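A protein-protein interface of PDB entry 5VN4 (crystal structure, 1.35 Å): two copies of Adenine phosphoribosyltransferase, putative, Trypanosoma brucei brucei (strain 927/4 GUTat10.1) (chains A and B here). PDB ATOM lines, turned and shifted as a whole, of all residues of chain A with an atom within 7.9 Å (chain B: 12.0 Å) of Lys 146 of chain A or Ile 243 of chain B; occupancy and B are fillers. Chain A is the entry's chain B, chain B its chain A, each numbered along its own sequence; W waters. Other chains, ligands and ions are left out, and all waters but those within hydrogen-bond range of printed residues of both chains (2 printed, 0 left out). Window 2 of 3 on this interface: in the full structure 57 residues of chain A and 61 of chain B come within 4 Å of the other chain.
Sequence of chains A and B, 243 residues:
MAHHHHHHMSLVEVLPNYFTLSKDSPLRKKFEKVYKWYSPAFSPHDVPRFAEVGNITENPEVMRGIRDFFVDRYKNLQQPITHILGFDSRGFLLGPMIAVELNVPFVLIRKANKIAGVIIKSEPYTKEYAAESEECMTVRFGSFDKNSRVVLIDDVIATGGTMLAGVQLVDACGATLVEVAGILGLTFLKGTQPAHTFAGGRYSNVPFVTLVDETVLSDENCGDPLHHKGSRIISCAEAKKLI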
ATOM      1  N   PHE A 141     -11.677 -11.339 -14.438  1.00  0.00           N
ATOM      2  CA  PHE A 141     -12.988 -10.791 -14.146  1.00  0.00           C
ATOM      3  C   PHE A 141     -12.863  -9.287 -13.949  1.00  0.00           C
ATOM      4  O   PHE A 141     -11.951  -8.813 -13.263  1.00  0.00           O
ATOM      5  CB  PHE A 141     -13.553 -11.438 -12.881  1.00  0.00           C
ATOM      6  CG  PHE A 141     -14.947 -10.988 -12.561  1.00  0.00           C
ATOM      7  CD1 PHE A 141     -16.036 -11.600 -13.159  1.00  0.00           C
ATOM      8  CD2 PHE A 141     -15.169  -9.929 -11.692  1.00  0.00           C
ATOM      9  CE1 PHE A 141     -17.326 -11.176 -12.880  1.00  0.00           C
ATOM     10  CE2 PHE A 141     -16.457  -9.496 -11.409  1.00  0.00           C
ATOM     11  CZ  PHE A 141     -17.536 -10.121 -12.006  1.00  0.00           C
ATOM     12  N   PHE A 144     -13.852  -6.509 -18.777  1.00  0.00           N
ATOM     13  CA  PHE A 144     -14.890  -6.025 -19.683  1.00  0.00           C
ATOM     14  C   PHE A 144     -16.223  -6.489 -19.111  1.00  0.00           C
ATOM     15  O   PHE A 144     -16.260  -7.306 -18.188  1.00  0.00           O
ATOM     16  CB  PHE A 144     -14.657  -6.489 -21.129  1.00  0.00           C
ATOM     17  CG  PHE A 144     -14.779  -7.976 -21.322  1.00  0.00           C
ATOM     18  CD1 PHE A 144     -13.729  -8.819 -21.003  1.00  0.00           C
ATOM     19  CD2 PHE A 144     -15.944  -8.527 -21.827  1.00  0.00           C
ATOM     20  CE1 PHE A 144     -13.847 -10.188 -21.172  1.00  0.00           C
ATOM     21  CE2 PHE A 144     -16.068  -9.892 -22.002  1.00  0.00           C
ATOM     22  CZ  PHE A 144     -15.019 -10.725 -21.677  1.00  0.00           C
ATOM     23  N   ASP A 145     -17.322  -5.933 -19.622  1.00  0.00           N
ATOM     24  CA  ASP A 145     -18.623  -6.207 -19.004  1.00  0.00           C
ATOM     25  C   ASP A 145     -19.718  -6.236 -20.068  1.00  0.00           C
ATOM     26  O   ASP A 145     -19.447  -6.208 -21.272  1.00  0.00           O
ATOM     27  CB  ASP A 145     -18.903  -5.256 -17.829  1.00  0.00           C
ATOM     28  CG  ASP A 145     -19.033  -3.795 -18.252  1.00  0.00           C
ATOM     29  OD1 ASP A 145     -19.375  -3.514 -19.422  1.00  0.00           O
ATOM     30  OD2 ASP A 145     -18.805  -2.913 -17.392  1.00  0.00           O
ATOM     31  N   LYS A 146     -20.974  -6.271 -19.610  1.00  0.00           N
ATOM     32  CA  LYS A 146     -22.106  -6.427 -20.518  1.00  0.00           C
ATOM     33  C   LYS A 146     -22.278  -5.240 -21.457  1.00  0.00           C
ATOM     34  O   LYS A 146     -22.963  -5.367 -22.482  1.00  0.00           O
ATOM     35  CB  LYS A 146     -23.395  -6.660 -19.728  1.00  0.00           C
ATOM     36  CG  LYS A 146     -23.823  -5.467 -18.910  1.00  0.00           C
ATOM     37  CD  LYS A 146     -25.083  -5.779 -18.124  1.00  0.00           C
ATOM     38  CE  LYS A 146     -25.607  -4.551 -17.397  1.00  0.00           C
ATOM     39  NZ  LYS A 146     -26.915  -4.815 -16.725  1.00  0.00           N
ATOM     40  N   ASN A 147     -21.671  -4.099 -21.142  1.00  0.00           N
ATOM     41  CA  ASN A 147     -21.741  -2.919 -21.989  1.00  0.00           C
ATOM     42  C   ASN A 147     -20.586  -2.834 -22.971  1.00  0.00           C
ATOM     43  O   ASN A 147     -20.528  -1.885 -23.757  1.00  0.00           O
ATOM     44  CB  ASN A 147     -21.781  -1.653 -21.129  1.00  0.00           C
ATOM     45  CG  ASN A 147     -23.007  -1.596 -20.247  1.00  0.00           C
ATOM     46  OD1 ASN A 147     -24.122  -1.846 -20.700  1.00  0.00           O
ATOM     47  ND2 ASN A 147     -22.803  -1.292 -18.973  1.00  0.00           N
ATOM     48  N   SER A 148     -19.677  -3.803 -22.949  1.00  0.00           N
ATOM     49  CA  SER A 148     -18.515  -3.774 -23.822  1.00  0.00           C
ATOM     50  C   SER A 148     -18.867  -4.277 -25.220  1.00  0.00           C
ATOM     51  O   SER A 148     -19.802  -5.063 -25.413  1.00  0.00           O
ATOM     52  CB  SER A 148     -17.389  -4.622 -23.229  1.00  0.00           C
ATOM     53  OG  SER A 148     -17.086  -4.195 -21.913  1.00  0.00           O
ATOM     54  N   ARG A 149     -18.093  -3.808 -26.199  1.00  0.00           N
ATOM     55  CA  ARG A 149     -18.209  -4.213 -27.599  1.00  0.00           C
ATOM     56  C   ARG A 149     -16.808  -4.668 -27.981  1.00  0.00           C
ATOM     57  O   ARG A 149     -15.897  -3.843 -28.101  1.00  0.00           O
ATOM     58  CB  ARG A 149     -18.685  -3.040 -28.460  1.00  0.00           C
ATOM     59  CG  ARG A 149     -20.061  -2.509 -28.057  1.00  0.00           C
ATOM     60  CD  ARG A 149     -20.603  -1.509 -29.075  1.00  0.00           C
ATOM     61  NE  ARG A 149     -20.933  -2.161 -30.343  1.00  0.00           N
ATOM     62  CZ  ARG A 149     -22.079  -2.791 -30.592  1.00  0.00           C
ATOM     63  NH1 ARG A 149     -23.037  -2.852 -29.672  1.00  0.00           N
ATOM     64  NH2 ARG A 149     -22.267  -3.369 -31.770  1.00  0.00           N
ATOM     65  N   LEU A 169     -15.943 -16.967 -22.940  1.00  0.00           N
ATOM     66  CA  LEU A 169     -15.573 -15.957 -21.951  1.00  0.00           C
ATOM     67  C   LEU A 169     -16.290 -14.634 -22.201  1.00  0.00           C
ATOM     68  O   LEU A 169     -16.692 -13.950 -21.253  1.00  0.00           O
ATOM     69  CB  LEU A 169     -14.057 -15.780 -21.947  1.00  0.00           C
ATOM     70  CG  LEU A 169     -13.286 -17.037 -21.519  1.00  0.00           C
ATOM     71  CD1 LEU A 169     -11.780 -16.888 -21.751  1.00  0.00           C
ATOM     72  CD2 LEU A 169     -13.574 -17.395 -20.057  1.00  0.00           C
ATOM     73  N   VAL A 170     -16.441 -14.246 -23.466  1.00  0.00           N
ATOM     74  CA  VAL A 170     -17.213 -13.048 -23.793  1.00  0.00           C
ATOM     75  C   VAL A 170     -18.657 -13.218 -23.348  1.00  0.00           C
ATOM     76  O   VAL A 170     -19.249 -12.330 -22.715  1.00  0.00           O
ATOM     77  CB  VAL A 170     -17.107 -12.747 -25.298  1.00  0.00           C
ATOM     78  CG1 VAL A 170     -18.036 -11.606 -25.694  1.00  0.00           C
ATOM     79  CG2 VAL A 170     -15.667 -12.415 -25.652  1.00  0.00           C
ATOM     80  N   ASP A 171     -19.236 -14.376 -23.666  1.00  0.00           N
ATOM     81  CA  ASP A 171     -20.606 -14.683 -23.277  1.00  0.00           C
ATOM     82  C   ASP A 171     -20.776 -14.670 -21.761  1.00  0.00           C
ATOM     83  O   ASP A 171     -21.824 -14.244 -21.255  1.00  0.00           O
ATOM     84  CB  ASP A 171     -20.963 -16.050 -23.857  1.00  0.00           C
ATOM     85  CG  ASP A 171     -22.382 -16.460 -23.566  1.00  0.00           C
ATOM     86  OD1 ASP A 171     -23.293 -16.059 -24.317  1.00  0.00           O
ATOM     87  OD2 ASP A 171     -22.578 -17.217 -22.598  1.00  0.00           O
ATOM     88  N   ALA A 172     -19.755 -15.118 -21.018  1.00  0.00           N
ATOM     89  CA  ALA A 172     -19.835 -15.166 -19.560  1.00  0.00           C
ATOM     90  C   ALA A 172     -19.961 -13.785 -18.938  1.00  0.00           C
ATOM     91  O   ALA A 172     -20.368 -13.681 -17.777  1.00  0.00           O
ATOM     92  CB  ALA A 172     -18.605 -15.870 -18.985  1.00  0.00           C
ATOM     93  N   CYS A 173     -19.610 -12.730 -19.671  1.00  0.00           N
ATOM     94  CA  CYS A 173     -19.769 -11.365 -19.192  1.00  0.00           C
ATOM     95  C   CYS A 173     -20.907 -10.627 -19.882  1.00  0.00           C
ATOM     96  O   CYS A 173     -21.121  -9.443 -19.598  1.00  0.00           O
ATOM     97  CB  CYS A 173     -18.464 -10.580 -19.361  1.00  0.00           C
ATOM     98  SG  CYS A 173     -17.079 -11.257 -18.445  1.00  0.00           S
ATOM     99  N   GLY A 174     -21.631 -11.285 -20.788  1.00  0.00           N
ATOM    100  CA  GLY A 174     -22.751 -10.648 -21.454  1.00  0.00           C
ATOM    101  C   GLY A 174     -22.378  -9.571 -22.448  1.00  0.00           C
ATOM    102  O   GLY A 174     -23.239  -8.776 -22.838  1.00  0.00           O
ATOM    103  N   ALA A 175     -21.121  -9.528 -22.878  1.00  0.00           N
ATOM    104  CA  ALA A 175     -20.656  -8.483 -23.773  1.00  0.00           C
ATOM    105  C   ALA A 175     -21.110  -8.748 -25.206  1.00  0.00           C
ATOM    106  O   ALA A 175     -21.508  -9.858 -25.573  1.00  0.00           O
ATOM    107  CB  ALA A 175     -19.130  -8.372 -23.732  1.00  0.00           C
ATOM    108  N   THR A 176     -21.063  -7.699 -26.018  1.00  0.00           N
ATOM    109  CA  THR A 176     -21.361  -7.816 -27.440  1.00  0.00           C
ATOM    110  C   THR A 176     -20.078  -8.197 -28.167  1.00  0.00           C
ATOM    111  O   THR A 176     -19.074  -7.478 -28.082  1.00  0.00           O
ATOM    112  CB  THR A 176     -21.893  -6.493 -27.981  1.00  0.00           C
ATOM    113  OG1 THR A 176     -23.147  -6.195 -27.359  1.00  0.00           O
ATOM    114  CG2 THR A 176     -22.090  -6.571 -29.494  1.00  0.00           C
ATOM    115  N   ILE B 234     -13.301 -18.894 -11.341  1.00  0.00           N
ATOM    116  CA  ILE B 234     -14.746 -19.084 -11.436  1.00  0.00           C
ATOM    117  C   ILE B 234     -15.115 -19.577 -12.832  1.00  0.00           C
ATOM    118  O   ILE B 234     -14.439 -19.274 -13.821  1.00  0.00           O
ATOM    119  CB  ILE B 234     -15.548 -17.820 -11.042  1.00  0.00           C
ATOM    120  CG1 ILE B 234     -15.434 -16.723 -12.103  1.00  0.00           C
ATOM    121  CG2 ILE B 234     -15.084 -17.308  -9.681  1.00  0.00           C
ATOM    122  CD1 ILE B 234     -16.328 -15.516 -11.800  1.00  0.00           C
ATOM    123  N   SER B 235     -16.197 -20.347 -12.903  1.00  0.00           N
ATOM    124  CA  SER B 235     -16.647 -20.885 -14.174  1.00  0.00           C
ATOM    125  C   SER B 235     -17.447 -19.840 -14.949  1.00  0.00           C
ATOM    126  O   SER B 235     -17.842 -18.798 -14.418  1.00  0.00           O
ATOM    127  CB  SER B 235     -17.535 -22.101 -13.945  1.00  0.00           C
ATOM    128  OG  SER B 235     -18.756 -21.690 -13.365  1.00  0.00           O
ATOM    129  N   CYS B 236     -17.693 -20.133 -16.230  1.00  0.00           N
ATOM    130  CA  CYS B 236     -18.552 -19.257 -17.023  1.00  0.00           C
ATOM    131  C   CYS B 236     -19.942 -19.149 -16.413  1.00  0.00           C
ATOM    132  O   CYS B 236     -20.506 -18.051 -16.338  1.00  0.00           O
ATOM    133  CB  CYS B 236     -18.633 -19.742 -18.473  1.00  0.00           C
ATOM    134  SG  CYS B 236     -17.129 -19.393 -19.420  1.00  0.00           S
ATOM    135  N   ALA B 237     -20.504 -20.272 -15.961  1.00  0.00           N
ATOM    136  CA  ALA B 237     -21.835 -20.239 -15.360  1.00  0.00           C
ATOM    137  C   ALA B 237     -21.845 -19.405 -14.085  1.00  0.00           C
ATOM    138  O   ALA B 237     -22.788 -18.643 -13.837  1.00  0.00           O
ATOM    139  CB  ALA B 237     -22.333 -21.659 -15.078  1.00  0.00           C
ATOM    140  N   GLU B 238     -20.801 -19.536 -13.259  1.00  0.00           N
ATOM    141  CA  GLU B 238     -20.711 -18.715 -12.054  1.00  0.00           C
ATOM    142  C   GLU B 238     -20.579 -17.240 -12.413  1.00  0.00           C
ATOM    143  O   GLU B 238     -21.248 -16.386 -11.819  1.00  0.00           O
ATOM    144  CB  GLU B 238     -19.543 -19.187 -11.176  1.00  0.00           C
ATOM    145  CG  GLU B 238     -19.746 -20.595 -10.589  1.00  0.00           C
ATOM    146  CD  GLU B 238     -18.505 -21.201  -9.912  1.00  0.00           C
ATOM    147  OE1 GLU B 238     -18.691 -22.105  -9.069  1.00  0.00           O
ATOM    148  OE2 GLU B 238     -17.357 -20.802 -10.215  1.00  0.00           O
ATOM    149  N   ALA B 239     -19.747 -16.923 -13.411  1.00  0.00           N
ATOM    150  CA  ALA B 239     -19.579 -15.532 -13.820  1.00  0.00           C
ATOM    151  C   ALA B 239     -20.886 -14.929 -14.336  1.00  0.00           C
ATOM    152  O   ALA B 239     -21.179 -13.755 -14.078  1.00  0.00           O
ATOM    153  CB  ALA B 239     -18.473 -15.428 -14.871  1.00  0.00           C
ATOM    154  N   LYS B 240     -21.691 -15.718 -15.057  1.00  0.00           N
ATOM    155  CA  LYS B 240     -22.929 -15.182 -15.617  1.00  0.00           C
ATOM    156  C   LYS B 240     -23.892 -14.717 -14.533  1.00  0.00           C
ATOM    157  O   LYS B 240     -24.674 -13.786 -14.760  1.00  0.00           O
ATOM    158  CB  LYS B 240     -23.596 -16.217 -16.523  1.00  0.00           C
ATOM    159  CG  LYS B 240     -22.867 -16.431 -17.832  1.00  0.00           C
ATOM    160  CD  LYS B 240     -23.518 -17.515 -18.670  1.00  0.00           C
ATOM    161  CE  LYS B 240     -24.274 -16.923 -19.848  1.00  0.00           C
ATOM    162  NZ  LYS B 240     -24.694 -17.982 -20.804  1.00  0.00           N
ATOM    163  N   LYS B 241     -23.860 -15.346 -13.358  1.00  0.00           N
ATOM    164  CA  LYS B 241     -24.746 -14.922 -12.280  1.00  0.00           C
ATOM    165  C   LYS B 241     -24.393 -13.538 -11.758  1.00  0.00           C
ATOM    166  O   LYS B 241     -25.214 -12.918 -11.072  1.00  0.00           O
ATOM    167  CB  LYS B 241     -24.703 -15.941 -11.143  1.00  0.00           C
ATOM    168  CG  LYS B 241     -25.216 -17.306 -11.545  1.00  0.00           C
ATOM    169  CD  LYS B 241     -25.175 -18.273 -10.383  1.00  0.00           C
ATOM    170  CE  LYS B 241     -25.655 -19.646 -10.812  1.00  0.00           C
ATOM    171  NZ  LYS B 241     -25.291 -20.687  -9.809  1.00  0.00           N
ATOM    172  N   LEU B 242     -23.199 -13.042 -12.075  1.00  0.00           N
ATOM    173  CA  LEU B 242     -22.732 -11.743 -11.617  1.00  0.00           C
ATOM    174  C   LEU B 242     -22.976 -10.632 -12.628  1.00  0.00           C
ATOM    175  O   LEU B 242     -22.669  -9.471 -12.336  1.00  0.00           O
ATOM    176  CB  LEU B 242     -21.238 -11.814 -11.281  1.00  0.00           C
ATOM    177  CG  LEU B 242     -20.822 -12.904 -10.289  1.00  0.00           C
ATOM    178  CD1 LEU B 242     -19.311 -12.969 -10.184  1.00  0.00           C
ATOM    179  CD2 LEU B 242     -21.451 -12.667  -8.919  1.00  0.00           C
ATOM    180  N   ILE B 243     -23.509 -10.952 -13.804  1.00  0.00           N
ATOM    181  CA  ILE B 243     -23.786  -9.946 -14.823  1.00  0.00           C
ATOM    182  C   ILE B 243     -24.782  -8.908 -14.310  1.00  0.00           C
ATOM    183  O   ILE B 243     -25.781  -9.249 -13.677  1.00  0.00           O
ATOM    184  CB  ILE B 243     -24.259 -10.596 -16.140  1.00  0.00           C
ATOM    185  CG1 ILE B 243     -23.124 -11.404 -16.773  1.00  0.00           C
ATOM    186  CG2 ILE B 243     -24.766  -9.540 -17.108  1.00  0.00           C
ATOM    187  CD1 ILE B 243     -23.549 -12.183 -18.000  1.00  0.00           C
ATOM    188  OXT ILE B 243     -24.606  -7.704 -14.513  1.00  0.00           O
HETATM  189  O   HOH W   1     -20.312 -18.600 -21.308  1.00  0.00           O
HETATM  190  O   HOH W   2     -19.563 -12.069 -15.522  1.00  0.00           O
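OD2 of Asp 171 of chain A is in salt-bridge range of NZ of Lys 240 of chain B (2.9 Å).
N of Lys 146 of chain A is in hydrogen-bond range of O of Cys 173 of chain A (3.2 Å).
Leu 242 of chain B touches Phe 141 of chain A (CD1 to CE1, 3.8 Å).
CD of Lys 146 of chain A touches CG2 of Ile 243 of chain B, 3.9 Å away.
Cys 236 of chain B touches Ala 172 of chain A.
Ala 239 of chain B touches Ala 172 of chain A (C to O, 3.7 Å).
Ala 172 of chain A touches Lys 240 of chain B (O to N, 3.6 Å).
CD1 of Ile 243 of chain B touches O of Ala 172 of chain A, 3.5 Å away.
Cys 173 of chain A touches Ile 243 of chain B (C to CD1, 3.6 Å).
Gly 174 of chain A touches Ile 243 of chain B.
Lys 146 of chain A touches just one residue of chain B: Ile 243 (3.9 Å).
Ile 243 of chain B touches just these residues of chain A: Lys 146 (3.9 Å), Ala 172 (3.5 Å), Cys 173 (3.6 Å) and Gly 174 (3.5 Å).
Asp 145 of chain A touches none of the printed residues of chain B.
No residue of chain B comes within 4 Å of Ser 148 of chain A.
Of the printed residues of chain B, Cys 173 of chain A touches Ile 243 (3.6 Å).
Of chain B, only Ile 243 (3.5 Å) comes within 4 Å of Gly 174 of chain A.
No residue of chain B comes within 4 Å of Ala 175 of chain A.
Thr 176 of chain A touches none of the printed residues of chain B.
Printed residues of chain B within 4 Å of Ala 172 of chain A: Cys 236 (3.8 Å), Ala 239 (3.7 Å), Lys 240 (3.6 Å) and Ile 243 (3.5 Å).
Printed residues of chain B within 4 Å of Phe 141 of chain A: Leu 242 (3.8 Å).
Of the printed residues of chain A, Cys 236 of chain B touches Ala 172.
Of the printed residues of chain B, Asp 171 of chain A touches Lys 240 (2.9 Å).
Leu 169 of chain A touches none of the printed residues of chain B.
The nearest residue of chain B that does not touch Lys 146 of chain A is Leu 242 of chain B (7.3 Å).
Hydrophobic or aromatic side chains of chain A within 4 Å of the printed part of chain B: Phe 141 and Ala 172.
Among the printed residues, 9 pairs touch across the chains.
No position is printed for both chains.
Water W2 lies within hydrogen-bond range of the backbone carbonyl oxygen (O) of Ala 239 of chain B and the backbone carbonyl oxygen (O) of Ala 172 of chain A.
Water W1 bridges OD2 of Asp 171 of chain A and SG of Cys 236 of chain B.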
